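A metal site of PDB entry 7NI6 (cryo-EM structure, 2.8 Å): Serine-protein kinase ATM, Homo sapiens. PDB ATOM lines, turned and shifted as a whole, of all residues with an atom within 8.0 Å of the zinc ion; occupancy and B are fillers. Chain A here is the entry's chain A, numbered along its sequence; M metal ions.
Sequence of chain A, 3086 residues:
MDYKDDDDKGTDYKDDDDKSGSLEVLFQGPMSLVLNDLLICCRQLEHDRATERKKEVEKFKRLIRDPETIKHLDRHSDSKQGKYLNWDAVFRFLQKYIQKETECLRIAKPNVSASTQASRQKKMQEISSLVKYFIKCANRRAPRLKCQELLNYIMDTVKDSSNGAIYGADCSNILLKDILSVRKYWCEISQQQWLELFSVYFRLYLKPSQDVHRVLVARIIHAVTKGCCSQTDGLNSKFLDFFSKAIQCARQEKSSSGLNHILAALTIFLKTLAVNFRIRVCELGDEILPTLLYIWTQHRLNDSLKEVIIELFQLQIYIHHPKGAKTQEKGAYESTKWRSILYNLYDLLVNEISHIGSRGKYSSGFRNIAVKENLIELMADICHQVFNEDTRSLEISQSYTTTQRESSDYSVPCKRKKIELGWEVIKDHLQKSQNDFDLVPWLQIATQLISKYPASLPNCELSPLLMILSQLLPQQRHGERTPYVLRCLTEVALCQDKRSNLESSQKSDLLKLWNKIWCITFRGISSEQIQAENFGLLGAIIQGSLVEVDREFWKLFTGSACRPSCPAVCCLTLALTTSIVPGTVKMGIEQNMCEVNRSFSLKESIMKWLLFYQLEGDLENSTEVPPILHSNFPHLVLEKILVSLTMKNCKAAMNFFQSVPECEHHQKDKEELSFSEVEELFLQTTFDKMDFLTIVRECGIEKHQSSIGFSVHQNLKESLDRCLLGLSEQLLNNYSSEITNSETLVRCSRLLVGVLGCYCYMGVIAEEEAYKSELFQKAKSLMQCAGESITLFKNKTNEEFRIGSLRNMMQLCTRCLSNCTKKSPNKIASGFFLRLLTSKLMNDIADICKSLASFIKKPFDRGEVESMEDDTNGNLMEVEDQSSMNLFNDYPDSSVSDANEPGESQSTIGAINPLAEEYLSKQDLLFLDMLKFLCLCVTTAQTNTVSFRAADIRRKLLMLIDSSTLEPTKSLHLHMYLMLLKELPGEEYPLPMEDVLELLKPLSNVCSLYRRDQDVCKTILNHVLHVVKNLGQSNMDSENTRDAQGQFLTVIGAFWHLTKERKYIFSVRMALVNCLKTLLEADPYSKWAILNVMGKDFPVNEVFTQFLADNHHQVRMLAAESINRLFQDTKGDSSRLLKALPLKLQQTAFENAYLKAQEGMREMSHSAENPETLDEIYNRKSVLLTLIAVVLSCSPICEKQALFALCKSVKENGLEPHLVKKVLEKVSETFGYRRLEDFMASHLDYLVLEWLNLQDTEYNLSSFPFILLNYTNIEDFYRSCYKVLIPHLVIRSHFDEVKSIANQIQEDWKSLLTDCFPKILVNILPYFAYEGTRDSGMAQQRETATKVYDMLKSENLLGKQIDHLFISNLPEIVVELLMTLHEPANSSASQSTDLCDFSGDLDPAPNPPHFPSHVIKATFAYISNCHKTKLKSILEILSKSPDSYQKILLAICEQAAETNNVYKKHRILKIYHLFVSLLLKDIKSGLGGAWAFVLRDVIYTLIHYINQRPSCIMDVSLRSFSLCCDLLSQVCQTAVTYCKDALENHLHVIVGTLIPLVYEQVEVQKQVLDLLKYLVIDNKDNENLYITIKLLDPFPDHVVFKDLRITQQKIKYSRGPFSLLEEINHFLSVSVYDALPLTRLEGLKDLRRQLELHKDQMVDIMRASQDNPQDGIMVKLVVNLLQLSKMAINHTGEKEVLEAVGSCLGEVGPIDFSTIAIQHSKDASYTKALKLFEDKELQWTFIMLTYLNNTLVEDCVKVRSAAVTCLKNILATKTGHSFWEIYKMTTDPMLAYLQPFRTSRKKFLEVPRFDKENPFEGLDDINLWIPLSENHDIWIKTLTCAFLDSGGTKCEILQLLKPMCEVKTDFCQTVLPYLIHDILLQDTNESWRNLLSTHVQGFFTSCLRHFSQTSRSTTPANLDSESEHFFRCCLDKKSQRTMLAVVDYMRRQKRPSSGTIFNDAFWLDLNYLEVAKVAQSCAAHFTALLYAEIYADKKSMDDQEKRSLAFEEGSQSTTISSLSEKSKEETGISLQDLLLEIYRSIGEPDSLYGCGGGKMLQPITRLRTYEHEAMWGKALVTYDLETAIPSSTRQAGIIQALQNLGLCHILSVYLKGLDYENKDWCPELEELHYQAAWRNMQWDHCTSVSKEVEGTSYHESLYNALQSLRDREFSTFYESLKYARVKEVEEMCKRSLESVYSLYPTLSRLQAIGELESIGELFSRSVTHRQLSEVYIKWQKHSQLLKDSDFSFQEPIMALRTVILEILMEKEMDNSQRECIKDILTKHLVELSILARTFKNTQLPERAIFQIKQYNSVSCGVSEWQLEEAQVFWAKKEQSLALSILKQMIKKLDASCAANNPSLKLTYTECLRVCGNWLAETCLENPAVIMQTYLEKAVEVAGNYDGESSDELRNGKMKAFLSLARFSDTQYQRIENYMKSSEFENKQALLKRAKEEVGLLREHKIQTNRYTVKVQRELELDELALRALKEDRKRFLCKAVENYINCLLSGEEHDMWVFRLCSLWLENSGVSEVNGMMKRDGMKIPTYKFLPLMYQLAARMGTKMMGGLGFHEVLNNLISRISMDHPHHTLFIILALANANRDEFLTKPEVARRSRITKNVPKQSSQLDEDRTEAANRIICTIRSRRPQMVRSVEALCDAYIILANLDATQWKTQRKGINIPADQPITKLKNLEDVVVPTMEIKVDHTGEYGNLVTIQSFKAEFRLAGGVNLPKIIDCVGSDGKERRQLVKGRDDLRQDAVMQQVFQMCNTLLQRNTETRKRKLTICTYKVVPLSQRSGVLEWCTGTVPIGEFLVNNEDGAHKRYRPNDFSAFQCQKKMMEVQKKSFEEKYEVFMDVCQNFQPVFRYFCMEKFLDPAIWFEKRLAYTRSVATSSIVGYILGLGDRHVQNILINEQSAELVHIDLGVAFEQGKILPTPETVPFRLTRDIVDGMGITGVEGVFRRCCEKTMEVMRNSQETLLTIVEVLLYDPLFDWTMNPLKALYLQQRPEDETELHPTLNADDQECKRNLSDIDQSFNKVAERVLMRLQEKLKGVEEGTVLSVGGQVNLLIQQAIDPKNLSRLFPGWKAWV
The side-chain sulfur (SG) of Cys 1929 sits close to the backbone NH (N) of Phe 1926 (3.3 Å).
Within 4 Å of the zinc ion: His 1906, His 1925, Cys 1929 and Cys 1930.
The nearest printed residue that does not touch the zinc ion is Phe 1926 (4.2 Å).
The zinc ion is bound by NE2 of His 1906 (2.0 Å), ND1 of His 1925 (2.0 Å), SG of Cys 1929 (2.3 Å) and SG of Cys 1930 (2.3 Å).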
ATOM      1  N   SER A1829      -1.855  -5.324 -15.933  1.00  0.00           N
ATOM      2  CA  SER A1829      -2.494  -6.582 -15.564  1.00  0.00           C
ATOM      3  C   SER A1829      -3.994  -6.517 -15.820  1.00  0.00           C
ATOM      4  O   SER A1829      -4.585  -7.473 -16.343  1.00  0.00           O
ATOM      5  CB  SER A1829      -2.205  -6.905 -14.096  1.00  0.00           C
ATOM      6  OG  SER A1829      -2.694  -5.885 -13.248  1.00  0.00           O
ATOM      7  N   SER A1902       7.112  -9.903 -22.999  1.00  0.00           N
ATOM      8  CA  SER A1902       6.556  -9.414 -21.750  1.00  0.00           C
ATOM      9  C   SER A1902       5.553 -10.391 -21.147  1.00  0.00           C
ATOM     10  O   SER A1902       5.417 -10.477 -19.929  1.00  0.00           O
ATOM     11  CB  SER A1902       5.901  -8.042 -21.954  1.00  0.00           C
ATOM     12  OG  SER A1902       5.335  -7.556 -20.749  1.00  0.00           O
ATOM     13  N   ARG A1905       7.346 -13.237 -18.752  1.00  0.00           N
ATOM     14  CA  ARG A1905       8.100 -12.981 -17.535  1.00  0.00           C
ATOM     15  C   ARG A1905       7.548 -13.827 -16.391  1.00  0.00           C
ATOM     16  O   ARG A1905       6.553 -14.542 -16.523  1.00  0.00           O
ATOM     17  CB  ARG A1905       8.073 -11.491 -17.184  1.00  0.00           C
ATOM     18  CG  ARG A1905       8.878 -10.626 -18.134  1.00  0.00           C
ATOM     19  CD  ARG A1905       8.818  -9.164 -17.744  1.00  0.00           C
ATOM     20  NE  ARG A1905       9.551  -8.309 -18.673  1.00  0.00           N
ATOM     21  CZ  ARG A1905       9.591  -6.997 -18.607  1.00  0.00           C
ATOM     22  NH1 ARG A1905       8.963  -6.328 -17.660  1.00  0.00           N
ATOM     23  NH2 ARG A1905      10.291  -6.321 -19.514  1.00  0.00           N
ATOM     24  N   HIS A1906       8.232 -13.742 -15.247  1.00  0.00           N
ATOM     25  CA  HIS A1906       7.918 -14.552 -14.077  1.00  0.00           C
ATOM     26  C   HIS A1906       7.994 -16.046 -14.399  1.00  0.00           C
ATOM     27  O   HIS A1906       8.789 -16.464 -15.248  1.00  0.00           O
ATOM     28  CB  HIS A1906       6.534 -14.214 -13.508  1.00  0.00           C
ATOM     29  CG  HIS A1906       6.370 -12.768 -13.136  1.00  0.00           C
ATOM     30  ND1 HIS A1906       6.891 -12.237 -11.974  1.00  0.00           N
ATOM     31  CD2 HIS A1906       5.735 -11.757 -13.766  1.00  0.00           C
ATOM     32  CE1 HIS A1906       6.582 -10.956 -11.915  1.00  0.00           C
ATOM     33  NE2 HIS A1906       5.892 -10.633 -12.987  1.00  0.00           N
ATOM     34  N   HIS A1925       6.691  -7.617  -8.661  1.00  0.00           N
ATOM     35  CA  HIS A1925       6.504  -7.914 -10.079  1.00  0.00           C
ATOM     36  C   HIS A1925       7.284  -6.938 -10.948  1.00  0.00           C
ATOM     37  O   HIS A1925       7.767  -5.909 -10.466  1.00  0.00           O
ATOM     38  CB  HIS A1925       5.020  -7.874 -10.444  1.00  0.00           C
ATOM     39  CG  HIS A1925       4.211  -8.993  -9.853  1.00  0.00           C
ATOM     40  ND1 HIS A1925       3.976 -10.167 -10.522  1.00  0.00           N
ATOM     41  CD2 HIS A1925       3.604  -9.117  -8.651  1.00  0.00           C
ATOM     42  CE1 HIS A1925       3.253 -10.969  -9.758  1.00  0.00           C
ATOM     43  NE2 HIS A1925       3.019 -10.347  -8.618  1.00  0.00           N
ATOM     44  N   PHE A1926       7.404  -7.263 -12.234  1.00  0.00           N
ATOM     45  CA  PHE A1926       8.149  -6.426 -13.164  1.00  0.00           C
ATOM     46  C   PHE A1926       7.322  -5.207 -13.570  1.00  0.00           C
ATOM     47  O   PHE A1926       6.178  -5.027 -13.149  1.00  0.00           O
ATOM     48  CB  PHE A1926       8.572  -7.232 -14.388  1.00  0.00           C
ATOM     49  CG  PHE A1926       9.486  -8.382 -14.066  1.00  0.00           C
ATOM     50  CD1 PHE A1926      10.855  -8.191 -13.977  1.00  0.00           C
ATOM     51  CD2 PHE A1926       8.976  -9.659 -13.871  1.00  0.00           C
ATOM     52  CE1 PHE A1926      11.698  -9.246 -13.680  1.00  0.00           C
ATOM     53  CE2 PHE A1926       9.814 -10.718 -13.582  1.00  0.00           C
ATOM     54  CZ  PHE A1926      11.172 -10.518 -13.489  1.00  0.00           C
ATOM     55  N   PHE A1927       7.927  -4.348 -14.387  1.00  0.00           N
ATOM     56  CA  PHE A1927       7.238  -3.135 -14.845  1.00  0.00           C
ATOM     57  C   PHE A1927       6.018  -3.482 -15.683  1.00  0.00           C
ATOM     58  O   PHE A1927       4.954  -2.882 -15.531  1.00  0.00           O
ATOM     59  CB  PHE A1927       8.206  -2.254 -15.621  1.00  0.00           C
ATOM     60  CG  PHE A1927       7.550  -1.095 -16.310  1.00  0.00           C
ATOM     61  CD1 PHE A1927       6.836  -0.155 -15.586  1.00  0.00           C
ATOM     62  CD2 PHE A1927       7.649  -0.943 -17.689  1.00  0.00           C
ATOM     63  CE1 PHE A1927       6.232   0.912 -16.224  1.00  0.00           C
ATOM     64  CE2 PHE A1927       7.046   0.124 -18.327  1.00  0.00           C
ATOM     65  CZ  PHE A1927       6.334   1.055 -17.600  1.00  0.00           C
ATOM     66  N   ARG A1928       6.152  -4.461 -16.578  1.00  0.00           N
ATOM     67  CA  ARG A1928       5.065  -4.903 -17.441  1.00  0.00           C
ATOM     68  C   ARG A1928       5.104  -6.424 -17.519  1.00  0.00           C
ATOM     69  O   ARG A1928       5.960  -6.994 -18.192  1.00  0.00           O
ATOM     70  CB  ARG A1928       5.176  -4.289 -18.837  1.00  0.00           C
ATOM     71  CG  ARG A1928       4.895  -2.800 -18.889  1.00  0.00           C
ATOM     72  CD  ARG A1928       3.486  -2.471 -18.417  1.00  0.00           C
ATOM     73  NE  ARG A1928       3.267  -1.032 -18.308  1.00  0.00           N
ATOM     74  CZ  ARG A1928       2.804  -0.272 -19.302  1.00  0.00           C
ATOM     75  NH1 ARG A1928       2.499  -0.784 -20.481  1.00  0.00           N
ATOM     76  NH2 ARG A1928       2.644   1.028 -19.087  1.00  0.00           N
ATOM     77  N   CYS A1929       4.165  -7.081 -16.835  1.00  0.00           N
ATOM     78  CA  CYS A1929       4.089  -8.533 -16.800  1.00  0.00           C
ATOM     79  C   CYS A1929       2.723  -8.924 -16.256  1.00  0.00           C
ATOM     80  O   CYS A1929       1.904  -8.073 -15.907  1.00  0.00           O
ATOM     81  CB  CYS A1929       5.225  -9.144 -15.971  1.00  0.00           C
ATOM     82  SG  CYS A1929       5.178  -8.691 -14.220  1.00  0.00           S
ATOM     83  N   CYS A1930       2.488 -10.240 -16.180  1.00  0.00           N
ATOM     84  CA  CYS A1930       1.236 -10.802 -15.652  1.00  0.00           C
ATOM     85  C   CYS A1930       0.024 -10.245 -16.386  1.00  0.00           C
ATOM     86  O   CYS A1930      -0.976  -9.849 -15.781  1.00  0.00           O
ATOM     87  CB  CYS A1930       1.129 -10.562 -14.140  1.00  0.00           C
ATOM     88  SG  CYS A1930       2.455 -11.296 -13.165  1.00  0.00           S
ATOM     89  N   LEU A1931       0.123 -10.206 -17.715  1.00  0.00           N
ATOM     90  CA  LEU A1931      -0.980  -9.712 -18.535  1.00  0.00           C
ATOM     91  C   LEU A1931      -2.172 -10.667 -18.463  1.00  0.00           C
ATOM     92  O   LEU A1931      -2.023 -11.868 -18.256  1.00  0.00           O
ATOM     93  CB  LEU A1931      -0.528  -9.547 -19.981  1.00  0.00           C
ATOM     94  CG  LEU A1931       0.694  -8.658 -20.209  1.00  0.00           C
ATOM     95  CD1 LEU A1931       0.907  -8.392 -21.685  1.00  0.00           C
ATOM     96  CD2 LEU A1931       0.555  -7.354 -19.434  1.00  0.00           C
HETATM   97 ZN    ZN M   1       4.092  -9.808 -12.526  1.00  0.00          ZN
